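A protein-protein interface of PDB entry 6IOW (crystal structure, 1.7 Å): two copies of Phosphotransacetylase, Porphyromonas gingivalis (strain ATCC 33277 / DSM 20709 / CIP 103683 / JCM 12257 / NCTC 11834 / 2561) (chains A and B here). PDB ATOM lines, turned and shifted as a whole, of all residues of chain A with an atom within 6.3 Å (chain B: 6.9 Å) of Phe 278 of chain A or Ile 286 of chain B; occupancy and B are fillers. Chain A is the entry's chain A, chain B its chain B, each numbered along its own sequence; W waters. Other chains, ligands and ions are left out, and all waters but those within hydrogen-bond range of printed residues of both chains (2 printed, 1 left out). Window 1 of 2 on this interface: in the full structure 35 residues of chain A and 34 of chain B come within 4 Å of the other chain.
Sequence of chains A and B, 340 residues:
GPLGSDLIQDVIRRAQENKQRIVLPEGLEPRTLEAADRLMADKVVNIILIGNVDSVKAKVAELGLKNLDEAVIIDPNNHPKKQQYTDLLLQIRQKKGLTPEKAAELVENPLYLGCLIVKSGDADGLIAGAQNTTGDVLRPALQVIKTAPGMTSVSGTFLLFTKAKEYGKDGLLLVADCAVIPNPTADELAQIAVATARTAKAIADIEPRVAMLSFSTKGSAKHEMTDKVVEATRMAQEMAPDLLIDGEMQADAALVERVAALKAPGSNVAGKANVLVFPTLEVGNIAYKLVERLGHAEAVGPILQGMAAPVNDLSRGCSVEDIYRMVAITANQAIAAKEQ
OD1 of Asn 285 of chain B sits at hydrogen-bond distance from NE2 of Gln 250 of chain A, at 3.2 Å.
N of Ala 176 of chain A is in hydrogen-bond range of O of Leu 276 of chain A (3.1 Å). N of Phe 278 of chain A sits at hydrogen-bond distance from O of Ala 176 of chain A (2.9 Å). O of Val 277 of chain A lies within hydrogen-bond range of N of Leu 213 of chain A, at 3.0 Å. The backbone NH (N) of Ser 214 of chain A sits at hydrogen-bond distance from the backbone carbonyl oxygen (O) of Met 249 of chain A (3.0 Å). O of Cys 178 of chain B is in hydrogen-bond range of ND2 of Asn 285 of chain B, at 3.0 Å. The side-chain hydroxyl of Tyr 288 of chain B sits at hydrogen-bond distance from the side-chain amino group of Lys 289 of chain B, at 3.0 Å.
Among the printed residues, merely in contact across the chains: Leu 213 of chain A with Ile 286 of chain B (3.7 Å), Ser 214 of chain A with Ile 286 of chain B (3.8 Å), Phe 215 of chain A with Leu 281 of chain B (3.8 Å), Phe 215 of chain A with Glu 282 of chain B (3.6 Å), Phe 215 of chain A with Asn 285 of chain B (3.8 Å), Gln 250 of chain A with Lys 289 of chain B (3.997 Å), Ala 251 of chain A with Lys 289 of chain B (3.8 Å), Ala 251 of chain A with Leu 290 of chain B (3.7 Å), Leu 276 of chain A with Leu 290 of chain B (3.8 Å), Phe 278 of chain A with Ile 286 of chain B (3.9 Å), Phe 278 of chain A with Leu 290 of chain B (3.7 Å), Pro 279 of chain A with Glu 282 of chain B (3.4 Å), Pro 279 of chain A with Ile 286 of chain B (3.8 Å), Thr 280 of chain A with Glu 282 of chain B (3.8 Å), Val 283 of chain A with Glu 282 of chain B (3.7 Å), Val 283 of chain A with Val 283 of chain B (3.6 Å) and Val 283 of chain A with Ile 286 of chain B (3.7 Å).
Asp 177 of chain A touches none of the printed residues of chain B. Met 249 of chain A touches none of the printed residues of chain B. Printed residues of chain B within 4 Å of Leu 276 of chain A: Leu 290. Phe 278 of chain A touches just these residues of chain B: Ile 286 (3.9 Å) and Leu 290 (3.7 Å). Of the printed residues of chain A, Leu 281 of chain B touches Phe 215 (3.8 Å). Printed residues of chain A within 4 Å of Ile 286 of chain B: Leu 213 (3.7 Å), Ser 214 (3.8 Å), Phe 278 (3.9 Å), Pro 279 (3.8 Å) and Val 283 (3.7 Å). The nearest residue of chain B that does not touch Phe 278 of chain A is Glu 282 of chain B (6.8 Å).
Hydrophobic or aromatic side chains of chain A within 4 Å of the printed part of chain B: Leu 213, Phe 215, Ala 251, Leu 276, Phe 278, Pro 279 and Val 283. Hydrophobic or aromatic side chains of chain B that line the printed part of chain A: Leu 281, Val 283, Ile 286 and Leu 290. Along chain B the printed residues that touch a printed residue of chain A span positions 281 to 290. Among the printed residues, 18 pairs touch across the chains.
Val 283 of chain B touches its own counterpart, Val 283 of chain A.
Water W1 lies within hydrogen-bond range of OG of Ser 214 of chain A (2.6 Å), OE2 of Glu 282 of chain B (2.7 Å) and N of Phe 215 of chain A (3.4 Å). Water W2 lies within hydrogen-bond range of OD1 of Asn 285 of chain B (2.7 Å), O of Ser 214 of chain A (3.0 Å) and N of Ala 251 of chain A (3.0 Å).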
ATOM      1  N   VAL A 175      11.800  18.936 -30.101  1.00  0.00           N
ATOM      2  CA  VAL A 175      11.088  18.904 -28.829  1.00  0.00           C
ATOM      3  C   VAL A 175       9.886  19.846 -28.926  1.00  0.00           C
ATOM      4  O   VAL A 175       9.965  20.901 -29.545  1.00  0.00           O
ATOM      5  CB  VAL A 175      12.024  19.261 -27.662  1.00  0.00           C
ATOM      6  CG1 VAL A 175      13.207  18.308 -27.595  1.00  0.00           C
ATOM      7  CG2 VAL A 175      12.499  20.709 -27.711  1.00  0.00           C
ATOM      8  N   ALA A 176       8.775  19.433 -28.306  1.00  0.00           N
ATOM      9  CA  ALA A 176       7.505  20.151 -28.370  1.00  0.00           C
ATOM     10  C   ALA A 176       6.612  19.641 -27.246  1.00  0.00           C
ATOM     11  O   ALA A 176       6.857  18.547 -26.747  1.00  0.00           O
ATOM     12  CB  ALA A 176       6.860  19.923 -29.718  1.00  0.00           C
ATOM     13  N   ASP A 177       5.579  20.405 -26.844  1.00  0.00           N
ATOM     14  CA  ASP A 177       5.295  21.764 -27.276  1.00  0.00           C
ATOM     15  C   ASP A 177       5.938  22.721 -26.271  1.00  0.00           C
ATOM     16  O   ASP A 177       5.678  22.612 -25.070  1.00  0.00           O
ATOM     17  CB  ASP A 177       3.782  21.991 -27.315  1.00  0.00           C
ATOM     18  CG  ASP A 177       3.299  23.419 -27.486  1.00  0.00           C
ATOM     19  OD1 ASP A 177       4.108  24.304 -27.866  1.00  0.00           O
ATOM     20  OD2 ASP A 177       2.080  23.635 -27.276  1.00  0.00           O
ATOM     21  N   CYS A 178       6.774  23.641 -26.762  1.00  0.00           N
ATOM     22  CA  CYS A 178       7.593  24.482 -25.887  1.00  0.00           C
ATOM     23  C   CYS A 178       7.073  25.926 -25.849  1.00  0.00           C
ATOM     24  O   CYS A 178       7.720  26.780 -25.225  1.00  0.00           O
ATOM     25  CB  CYS A 178       9.048  24.475 -26.342  1.00  0.00           C
ATOM     26  SG  CYS A 178       9.788  22.826 -26.258  1.00  0.00           S
ATOM     27  N   PRO A 184      -1.907  20.471 -22.499  1.00  0.00           N
ATOM     28  CA  PRO A 184      -2.578  19.733 -23.568  1.00  0.00           C
ATOM     29  C   PRO A 184      -3.500  18.629 -23.028  1.00  0.00           C
ATOM     30  O   PRO A 184      -3.135  17.909 -22.090  1.00  0.00           O
ATOM     31  CB  PRO A 184      -1.423  19.125 -24.382  1.00  0.00           C
ATOM     32  CG  PRO A 184      -0.243  20.031 -24.085  1.00  0.00           C
ATOM     33  CD  PRO A 184      -0.446  20.489 -22.659  1.00  0.00           C
ATOM     34  N   LEU A 189      -2.162  16.442 -27.129  1.00  0.00           N
ATOM     35  CA  LEU A 189      -0.827  15.890 -26.968  1.00  0.00           C
ATOM     36  C   LEU A 189      -0.520  14.900 -28.103  1.00  0.00           C
ATOM     37  O   LEU A 189       0.598  14.848 -28.603  1.00  0.00           O
ATOM     38  CB  LEU A 189      -0.702  15.239 -25.587  1.00  0.00           C
ATOM     39  CG  LEU A 189       0.726  14.939 -25.130  1.00  0.00           C
ATOM     40  CD1 LEU A 189       1.579  16.202 -25.134  1.00  0.00           C
ATOM     41  CD2 LEU A 189       0.733  14.309 -23.749  1.00  0.00           C
ATOM     42  N   ILE A 192       0.337  16.945 -31.074  1.00  0.00           N
ATOM     43  CA  ILE A 192       1.729  17.433 -30.940  1.00  0.00           C
ATOM     44  C   ILE A 192       2.701  16.355 -31.420  1.00  0.00           C
ATOM     45  O   ILE A 192       3.643  16.655 -32.155  1.00  0.00           O
ATOM     46  CB  ILE A 192       2.047  17.875 -29.497  1.00  0.00           C
ATOM     47  CG1 ILE A 192       1.258  19.126 -29.104  1.00  0.00           C
ATOM     48  CG2 ILE A 192       3.542  18.076 -29.305  1.00  0.00           C
ATOM     49  CD1 ILE A 192       1.139  19.351 -27.622  1.00  0.00           C
ATOM     50  N   ALA A 211       9.112   9.851 -28.489  1.00  0.00           N
ATOM     51  CA  ALA A 211       8.957   9.460 -27.085  1.00  0.00           C
ATOM     52  C   ALA A 211       7.952  10.389 -26.404  1.00  0.00           C
ATOM     53  O   ALA A 211       8.156  11.614 -26.350  1.00  0.00           O
ATOM     54  CB  ALA A 211      10.289   9.496 -26.390  1.00  0.00           C
ATOM     55  N   MET A 212       6.861   9.795 -25.902  1.00  0.00           N
ATOM     56  CA  MET A 212       5.864  10.502 -25.123  1.00  0.00           C
ATOM     57  C   MET A 212       6.325  10.467 -23.663  1.00  0.00           C
ATOM     58  O   MET A 212       6.289   9.401 -23.031  1.00  0.00           O
ATOM     59  CB  MET A 212       4.488   9.841 -25.270  1.00  0.00           C
ATOM     60  CG  MET A 212       4.072   9.607 -26.720  1.00  0.00           C
ATOM     61  SD  MET A 212       3.761  11.139 -27.627  1.00  0.00           S
ATOM     62  CE  MET A 212       2.219  11.661 -26.884  1.00  0.00           C
ATOM     63  N   LEU A 213       6.818  11.609 -23.160  1.00  0.00           N
ATOM     64  CA  LEU A 213       7.595  11.624 -21.919  1.00  0.00           C
ATOM     65  C   LEU A 213       6.666  11.763 -20.710  1.00  0.00           C
ATOM     66  O   LEU A 213       5.568  12.307 -20.785  1.00  0.00           O
ATOM     67  CB  LEU A 213       8.608  12.768 -21.946  1.00  0.00           C
ATOM     68  CG  LEU A 213       9.760  12.638 -22.940  1.00  0.00           C
ATOM     69  CD1 LEU A 213      10.763  13.757 -22.720  1.00  0.00           C
ATOM     70  CD2 LEU A 213      10.439  11.288 -22.818  1.00  0.00           C
ATOM     71  N   SER A 214       7.176  11.271 -19.583  1.00  0.00           N
ATOM     72  CA  SER A 214       6.446  11.106 -18.354  1.00  0.00           C
ATOM     73  C   SER A 214       7.468  10.952 -17.225  1.00  0.00           C
ATOM     74  O   SER A 214       8.677  10.849 -17.497  1.00  0.00           O
ATOM     75  CB  SER A 214       5.527   9.906 -18.492  1.00  0.00           C
ATOM     76  OG  SER A 214       4.913   9.555 -17.263  1.00  0.00           O
ATOM     77  N   PHE A 215       7.001  10.964 -15.971  1.00  0.00           N
ATOM     78  CA  PHE A 215       7.834  10.538 -14.834  1.00  0.00           C
ATOM     79  C   PHE A 215       7.718   9.024 -14.624  1.00  0.00           C
ATOM     80  O   PHE A 215       8.413   8.463 -13.757  1.00  0.00           O
ATOM     81  CB  PHE A 215       7.497  11.310 -13.553  1.00  0.00           C
ATOM     82  CG  PHE A 215       6.065  11.224 -13.088  1.00  0.00           C
ATOM     83  CD1 PHE A 215       5.525  10.029 -12.633  1.00  0.00           C
ATOM     84  CD2 PHE A 215       5.279  12.364 -13.041  1.00  0.00           C
ATOM     85  CE1 PHE A 215       4.213   9.974 -12.188  1.00  0.00           C
ATOM     86  CE2 PHE A 215       3.968  12.306 -12.596  1.00  0.00           C
ATOM     87  CZ  PHE A 215       3.440  11.112 -12.165  1.00  0.00           C
ATOM     88  N   MET A 249       7.130   7.120 -21.237  1.00  0.00           N
ATOM     89  CA  MET A 249       8.469   6.780 -20.824  1.00  0.00           C
ATOM     90  C   MET A 249       9.205   8.003 -20.260  1.00  0.00           C
ATOM     91  O   MET A 249       8.967   9.151 -20.658  1.00  0.00           O
ATOM     92  CB  MET A 249       9.260   6.159 -21.980  1.00  0.00           C
ATOM     93  CG  MET A 249       9.639   7.119 -23.099  1.00  0.00           C
ATOM     94  SD  MET A 249      10.510   6.244 -24.432  1.00  0.00           S
ATOM     95  CE  MET A 249       9.164   5.278 -25.131  1.00  0.00           C
ATOM     96  N   GLN A 250      10.110   7.728 -19.316  1.00  0.00           N
ATOM     97  CA  GLN A 250      10.988   8.734 -18.737  1.00  0.00           C
ATOM     98  C   GLN A 250      12.048   9.137 -19.765  1.00  0.00           C
ATOM     99  O   GLN A 250      12.280   8.434 -20.740  1.00  0.00           O
ATOM    100  CB  GLN A 250      11.626   8.196 -17.457  1.00  0.00           C
ATOM    101  CG  GLN A 250      10.619   8.074 -16.322  1.00  0.00           C
ATOM    102  CD  GLN A 250      11.099   7.141 -15.242  1.00  0.00           C
ATOM    103  OE1 GLN A 250      11.081   5.921 -15.406  1.00  0.00           O
ATOM    104  NE2 GLN A 250      11.548   7.711 -14.133  1.00  0.00           N
ATOM    105  N   ALA A 251      12.690  10.277 -19.512  1.00  0.00           N
ATOM    106  CA  ALA A 251      13.640  10.871 -20.443  1.00  0.00           C
ATOM    107  C   ALA A 251      14.858   9.955 -20.626  1.00  0.00           C
ATOM    108  O   ALA A 251      15.430   9.901 -21.707  1.00  0.00           O
ATOM    109  CB  ALA A 251      14.050  12.239 -19.961  1.00  0.00           C
ATOM    110  N   LEU A 276      11.084  14.421 -28.768  1.00  0.00           N
ATOM    111  CA  LEU A 276      10.579  14.366 -27.397  1.00  0.00           C
ATOM    112  C   LEU A 276       9.296  15.195 -27.308  1.00  0.00           C
ATOM    113  O   LEU A 276       9.274  16.397 -27.673  1.00  0.00           O
ATOM    114  CB  LEU A 276      11.628  14.902 -26.416  1.00  0.00           C
ATOM    115  CG  LEU A 276      13.033  14.300 -26.506  1.00  0.00           C
ATOM    116  CD1 LEU A 276      13.929  14.914 -25.447  1.00  0.00           C
ATOM    117  CD2 LEU A 276      13.000  12.784 -26.376  1.00  0.00           C
ATOM    118  N   VAL A 277       8.239  14.554 -26.800  1.00  0.00           N
ATOM    119  CA  VAL A 277       6.944  15.182 -26.587  1.00  0.00           C
ATOM    120  C   VAL A 277       6.705  15.332 -25.084  1.00  0.00           C
ATOM    121  O   VAL A 277       6.596  14.331 -24.362  1.00  0.00           O
ATOM    122  CB  VAL A 277       5.827  14.366 -27.259  1.00  0.00           C
ATOM    123  CG1 VAL A 277       4.456  14.943 -26.957  1.00  0.00           C
ATOM    124  CG2 VAL A 277       6.060  14.265 -28.758  1.00  0.00           C
ATOM    125  N   PHE A 278       6.638  16.589 -24.634  1.00  0.00           N
ATOM    126  CA  PHE A 278       6.503  16.929 -23.231  1.00  0.00           C
ATOM    127  C   PHE A 278       5.021  16.950 -22.864  1.00  0.00           C
ATOM    128  O   PHE A 278       4.202  17.333 -23.682  1.00  0.00           O
ATOM    129  CB  PHE A 278       7.130  18.297 -22.956  1.00  0.00           C
ATOM    130  CG  PHE A 278       8.589  18.402 -23.309  1.00  0.00           C
ATOM    131  CD1 PHE A 278       9.516  17.569 -22.709  1.00  0.00           C
ATOM    132  CD2 PHE A 278       9.034  19.339 -24.227  1.00  0.00           C
ATOM    133  CE1 PHE A 278      10.864  17.674 -23.022  1.00  0.00           C
ATOM    134  CE2 PHE A 278      10.378  19.444 -24.538  1.00  0.00           C
ATOM    135  CZ  PHE A 278      11.291  18.613 -23.931  1.00  0.00           C
ATOM    136  N   PRO A 279       4.630  16.524 -21.641  1.00  0.00           N
ATOM    137  CA  PRO A 279       3.206  16.454 -21.289  1.00  0.00           C
ATOM    138  C   PRO A 279       2.511  17.790 -20.967  1.00  0.00           C
ATOM    139  O   PRO A 279       1.265  17.864 -21.054  1.00  0.00           O
ATOM    140  CB  PRO A 279       3.204  15.513 -20.074  1.00  0.00           C
ATOM    141  CG  PRO A 279       4.573  15.678 -19.453  1.00  0.00           C
ATOM    142  CD  PRO A 279       5.514  15.978 -20.600  1.00  0.00           C
ATOM    143  N   THR A 280       3.284  18.827 -20.618  1.00  0.00           N
ATOM    144  CA  THR A 280       2.755  20.190 -20.376  1.00  0.00           C
ATOM    145  C   THR A 280       3.769  21.241 -20.839  1.00  0.00           C
ATOM    146  O   THR A 280       4.948  20.936 -21.080  1.00  0.00           O
ATOM    147  CB  THR A 280       2.412  20.453 -18.902  1.00  0.00           C
ATOM    148  OG1 THR A 280       3.621  20.743 -18.191  1.00  0.00           O
ATOM    149  CG2 THR A 280       1.675  19.307 -18.248  1.00  0.00           C
ATOM    150  N   LEU A 281       3.299  22.494 -20.898  1.00  0.00           N
ATOM    151  CA  LEU A 281       4.125  23.632 -21.280  1.00  0.00           C
ATOM    152  C   LEU A 281       5.123  23.968 -20.164  1.00  0.00           C
ATOM    153  O   LEU A 281       6.191  24.507 -20.436  1.00  0.00           O
ATOM    154  CB  LEU A 281       3.222  24.821 -21.613  1.00  0.00           C
ATOM    155  CG  LEU A 281       3.932  26.097 -22.073  1.00  0.00           C
ATOM    156  CD1 LEU A 281       4.764  25.854 -23.321  1.00  0.00           C
ATOM    157  CD2 LEU A 281       2.926  27.205 -22.315  1.00  0.00           C
ATOM    158  N   VAL A 283       6.696  21.676 -18.511  1.00  0.00           N
ATOM    159  CA  VAL A 283       7.789  20.778 -18.857  1.00  0.00           C
ATOM    160  C   VAL A 283       8.544  21.344 -20.068  1.00  0.00           C
ATOM    161  O   VAL A 283       9.771  21.449 -20.034  1.00  0.00           O
ATOM    162  CB  VAL A 283       7.326  19.337 -19.133  1.00  0.00           C
ATOM    163  CG1 VAL A 283       8.522  18.471 -19.518  1.00  0.00           C
ATOM    164  CG2 VAL A 283       6.570  18.732 -17.952  1.00  0.00           C
ATOM    165  N   GLY A 284       7.809  21.678 -21.136  1.00  0.00           N
ATOM    166  CA  GLY A 284       8.434  22.041 -22.413  1.00  0.00           C
ATOM    167  C   GLY A 284       9.273  23.309 -22.310  1.00  0.00           C
ATOM    168  O   GLY A 284      10.420  23.357 -22.748  1.00  0.00           O
ATOM    169  N   ASN A 285       8.684  24.352 -21.723  1.00  0.00           N
ATOM    170  CA  ASN A 285       9.298  25.668 -21.659  1.00  0.00           C
ATOM    171  C   ASN A 285      10.526  25.639 -20.737  1.00  0.00           C
ATOM    172  O   ASN A 285      11.561  26.226 -21.072  1.00  0.00           O
ATOM    173  CB  ASN A 285       8.286  26.727 -21.212  1.00  0.00           C
ATOM    174  CG  ASN A 285       8.719  28.124 -21.573  1.00  0.00           C
ATOM    175  OD1 ASN A 285       9.167  28.875 -20.708  1.00  0.00           O
ATOM    176  ND2 ASN A 285       8.593  28.472 -22.847  1.00  0.00           N
ATOM    177  N   ALA A 287      12.302  22.780 -19.748  1.00  0.00           N
ATOM    178  CA  ALA A 287      13.300  21.771 -20.144  1.00  0.00           C
ATOM    179  C   ALA A 287      14.172  22.263 -21.306  1.00  0.00           C
ATOM    180  O   ALA A 287      15.404  22.109 -21.249  1.00  0.00           O
ATOM    181  CB  ALA A 287      12.645  20.451 -20.477  1.00  0.00           C
ATOM    182  N   TYR A 288      13.580  22.820 -22.368  1.00  0.00           N
ATOM    183  CA  TYR A 288      14.410  23.185 -23.536  1.00  0.00           C
ATOM    184  C   TYR A 288      15.360  24.328 -23.144  1.00  0.00           C
ATOM    185  O   TYR A 288      16.524  24.345 -23.550  1.00  0.00           O
ATOM    186  CB  TYR A 288      13.567  23.503 -24.776  1.00  0.00           C
ATOM    187  CG  TYR A 288      13.307  24.966 -25.020  1.00  0.00           C
ATOM    188  CD1 TYR A 288      14.229  25.759 -25.679  1.00  0.00           C
ATOM    189  CD2 TYR A 288      12.127  25.561 -24.608  1.00  0.00           C
ATOM    190  CE1 TYR A 288      13.983  27.101 -25.921  1.00  0.00           C
ATOM    191  CE2 TYR A 288      11.873  26.904 -24.830  1.00  0.00           C
ATOM    192  CZ  TYR A 288      12.804  27.680 -25.488  1.00  0.00           C
ATOM    193  OH  TYR A 288      12.538  29.002 -25.683  1.00  0.00           O
ATOM    194  N   CYS B 178      12.558  15.976  -7.905  1.00  0.00           N
ATOM    195  CA  CYS B 178      12.833  15.183  -9.101  1.00  0.00           C
ATOM    196  C   CYS B 178      12.455  13.710  -8.911  1.00  0.00           C
ATOM    197  O   CYS B 178      12.710  12.903  -9.814  1.00  0.00           O
ATOM    198  CB  CYS B 178      14.304  15.279  -9.485  1.00  0.00           C
ATOM    199  SG  CYS B 178      14.847  16.960  -9.872  1.00  0.00           S
ATOM    200  N   LEU B 281       6.401  16.854 -10.874  1.00  0.00           N
ATOM    201  CA  LEU B 281       7.365  15.776 -11.035  1.00  0.00           C
ATOM    202  C   LEU B 281       7.617  15.495 -12.522  1.00  0.00           C
ATOM    203  O   LEU B 281       8.698  15.030 -12.885  1.00  0.00           O
ATOM    204  CB  LEU B 281       6.842  14.526 -10.320  1.00  0.00           C
ATOM    205  CG  LEU B 281       7.772  13.312 -10.332  1.00  0.00           C
ATOM    206  CD1 LEU B 281       9.137  13.635  -9.753  1.00  0.00           C
ATOM    207  CD2 LEU B 281       7.132  12.156  -9.586  1.00  0.00           C
ATOM    208  N   GLU B 282       6.631  15.767 -13.383  1.00  0.00           N
ATOM    209  CA  GLU B 282       6.863  15.678 -14.829  1.00  0.00           C
ATOM    210  C   GLU B 282       7.991  16.645 -15.204  1.00  0.00           C
ATOM    211  O   GLU B 282       8.918  16.288 -15.925  1.00  0.00           O
ATOM    212  CB  GLU B 282       5.593  15.961 -15.624  1.00  0.00           C
ATOM    213  CG  GLU B 282       4.596  14.827 -15.543  1.00  0.00           C
ATOM    214  CD  GLU B 282       3.331  14.987 -16.365  1.00  0.00           C
ATOM    215  OE1 GLU B 282       2.864  16.133 -16.517  1.00  0.00           O
ATOM    216  OE2 GLU B 282       2.793  13.954 -16.809  1.00  0.00           O
ATOM    217  N   VAL B 283       7.919  17.873 -14.683  1.00  0.00           N
ATOM    218  CA  VAL B 283       8.965  18.836 -14.972  1.00  0.00           C
ATOM    219  C   VAL B 283      10.284  18.337 -14.377  1.00  0.00           C
ATOM    220  O   VAL B 283      11.309  18.306 -15.061  1.00  0.00           O
ATOM    221  CB  VAL B 283       8.651  20.250 -14.451  1.00  0.00           C
ATOM    222  CG1 VAL B 283       9.808  21.188 -14.756  1.00  0.00           C
ATOM    223  CG2 VAL B 283       7.353  20.797 -15.022  1.00  0.00           C
ATOM    224  N   GLY B 284      10.260  17.962 -13.094  1.00  0.00           N
ATOM    225  CA  GLY B 284      11.493  17.651 -12.373  1.00  0.00           C
ATOM    226  C   GLY B 284      12.219  16.445 -12.938  1.00  0.00           C
ATOM    227  O   GLY B 284      13.435  16.502 -13.182  1.00  0.00           O
ATOM    228  N   ASN B 285      11.466  15.365 -13.157  1.00  0.00           N
ATOM    229  CA  ASN B 285      12.022  14.092 -13.577  1.00  0.00           C
ATOM    230  C   ASN B 285      12.565  14.204 -15.012  1.00  0.00           C
ATOM    231  O   ASN B 285      13.644  13.704 -15.306  1.00  0.00           O
ATOM    232  CB  ASN B 285      10.996  12.964 -13.449  1.00  0.00           C
ATOM    233  CG  ASN B 285      11.638  11.598 -13.441  1.00  0.00           C
ATOM    234  OD1 ASN B 285      11.575  10.883 -14.441  1.00  0.00           O
ATOM    235  ND2 ASN B 285      12.249  11.235 -12.321  1.00  0.00           N
ATOM    236  N   ILE B 286      11.822  14.882 -15.897  1.00  0.00           N
ATOM    237  CA  ILE B 286      12.238  15.048 -17.306  1.00  0.00           C
ATOM    238  C   ILE B 286      13.428  16.019 -17.384  1.00  0.00           C
ATOM    239  O   ILE B 286      14.427  15.730 -18.035  1.00  0.00           O
ATOM    240  CB  ILE B 286      11.046  15.484 -18.189  1.00  0.00           C
ATOM    241  CG1 ILE B 286      10.001  14.368 -18.298  1.00  0.00           C
ATOM    242  CG2 ILE B 286      11.527  15.948 -19.562  1.00  0.00           C
ATOM    243  CD1 ILE B 286       8.664  14.799 -18.858  1.00  0.00           C
ATOM    244  N   ALA B 287      13.333  17.175 -16.715  1.00  0.00           N
ATOM    245  CA  ALA B 287      14.320  18.253 -16.916  1.00  0.00           C
ATOM    246  C   ALA B 287      15.716  17.858 -16.402  1.00  0.00           C
ATOM    247  O   ALA B 287      16.692  18.095 -17.093  1.00  0.00           O
ATOM    248  CB  ALA B 287      13.843  19.540 -16.290  1.00  0.00           C
ATOM    249  N   TYR B 288      15.830  17.255 -15.211  1.00  0.00           N
ATOM    250  CA  TYR B 288      17.183  16.960 -14.689  1.00  0.00           C
ATOM    251  C   TYR B 288      17.840  15.897 -15.579  1.00  0.00           C
ATOM    252  O   TYR B 288      19.038  15.967 -15.850  1.00  0.00           O
ATOM    253  CB  TYR B 288      17.171  16.566 -13.206  1.00  0.00           C
ATOM    254  CG  TYR B 288      17.187  15.083 -12.931  1.00  0.00           C
ATOM    255  CD1 TYR B 288      18.372  14.356 -12.945  1.00  0.00           C
ATOM    256  CD2 TYR B 288      16.012  14.403 -12.665  1.00  0.00           C
ATOM    257  CE1 TYR B 288      18.378  12.989 -12.711  1.00  0.00           C
ATOM    258  CE2 TYR B 288      15.999  13.042 -12.425  1.00  0.00           C
ATOM    259  CZ  TYR B 288      17.187  12.333 -12.446  1.00  0.00           C
ATOM    260  OH  TYR B 288      17.183  10.986 -12.212  1.00  0.00           O
ATOM    261  N   LYS B 289      17.047  14.922 -16.042  1.00  0.00           N
ATOM    262  CA  LYS B 289      17.556  13.820 -16.878  1.00  0.00           C
ATOM    263  C   LYS B 289      18.042  14.378 -18.226  1.00  0.00           C
ATOM    264  O   LYS B 289      19.090  13.973 -18.719  1.00  0.00           O
ATOM    265  CB  LYS B 289      16.488  12.740 -17.078  1.00  0.00           C
ATOM    266  CG  LYS B 289      16.246  11.825 -15.885  1.00  0.00           C
ATOM    267  CD  LYS B 289      15.158  10.789 -16.131  1.00  0.00           C
ATOM    268  CE  LYS B 289      14.675  10.086 -14.880  1.00  0.00           C
ATOM    269  NZ  LYS B 289      15.728   9.258 -14.260  1.00  0.00           N
ATOM    270  N   LEU B 290      17.287  15.315 -18.813  1.00  0.00           N
ATOM    271  CA  LEU B 290      17.698  15.905 -20.093  1.00  0.00           C
ATOM    272  C   LEU B 290      18.945  16.781 -19.916  1.00  0.00           C
ATOM    273  O   LEU B 290      19.810  16.764 -20.776  1.00  0.00           O
ATOM    274  CB  LEU B 290      16.537  16.680 -20.727  1.00  0.00           C
ATOM    275  CG  LEU B 290      15.353  15.830 -21.193  1.00  0.00           C
ATOM    276  CD1 LEU B 290      14.293  16.697 -21.863  1.00  0.00           C
ATOM    277  CD2 LEU B 290      15.790  14.703 -22.124  1.00  0.00           C
ATOM    278  N   VAL B 291      19.054  17.521 -18.805  1.00  0.00           N
ATOM    279  CA  VAL B 291      20.259  18.317 -18.551  1.00  0.00           C
ATOM    280  C   VAL B 291      21.463  17.373 -18.396  1.00  0.00           C
ATOM    281  O   VAL B 291      22.531  17.649 -18.932  1.00  0.00           O
ATOM    282  CB  VAL B 291      20.108  19.259 -17.341  1.00  0.00           C
ATOM    283  CG1 VAL B 291      21.430  19.913 -16.960  1.00  0.00           C
ATOM    284  CG2 VAL B 291      19.048  20.318 -17.597  1.00  0.00           C
ATOM    285  N   GLU B 292      21.263  16.255 -17.692  1.00  0.00           N
ATOM    286  CA  GLU B 292      22.297  15.241 -17.503  1.00  0.00           C
ATOM    287  C   GLU B 292      22.740  14.688 -18.864  1.00  0.00           C
ATOM    288  O   GLU B 292      23.926  14.745 -19.203  1.00  0.00           O
ATOM    289  CB  GLU B 292      21.778  14.128 -16.587  1.00  0.00           C
ATOM    290  CG  GLU B 292      22.800  13.047 -16.284  1.00  0.00           C
ATOM    291  CD  GLU B 292      22.255  11.841 -15.541  1.00  0.00           C
ATOM    292  OE1 GLU B 292      21.043  11.805 -15.253  1.00  0.00           O
ATOM    293  OE2 GLU B 292      23.060  10.936 -15.243  1.00  0.00           O
HETATM  294  O   HOH W   1       3.665  11.514 -16.136  1.00  0.00           O
HETATM  295  O   HOH W   2      11.535  11.523 -17.045  1.00  0.00           O
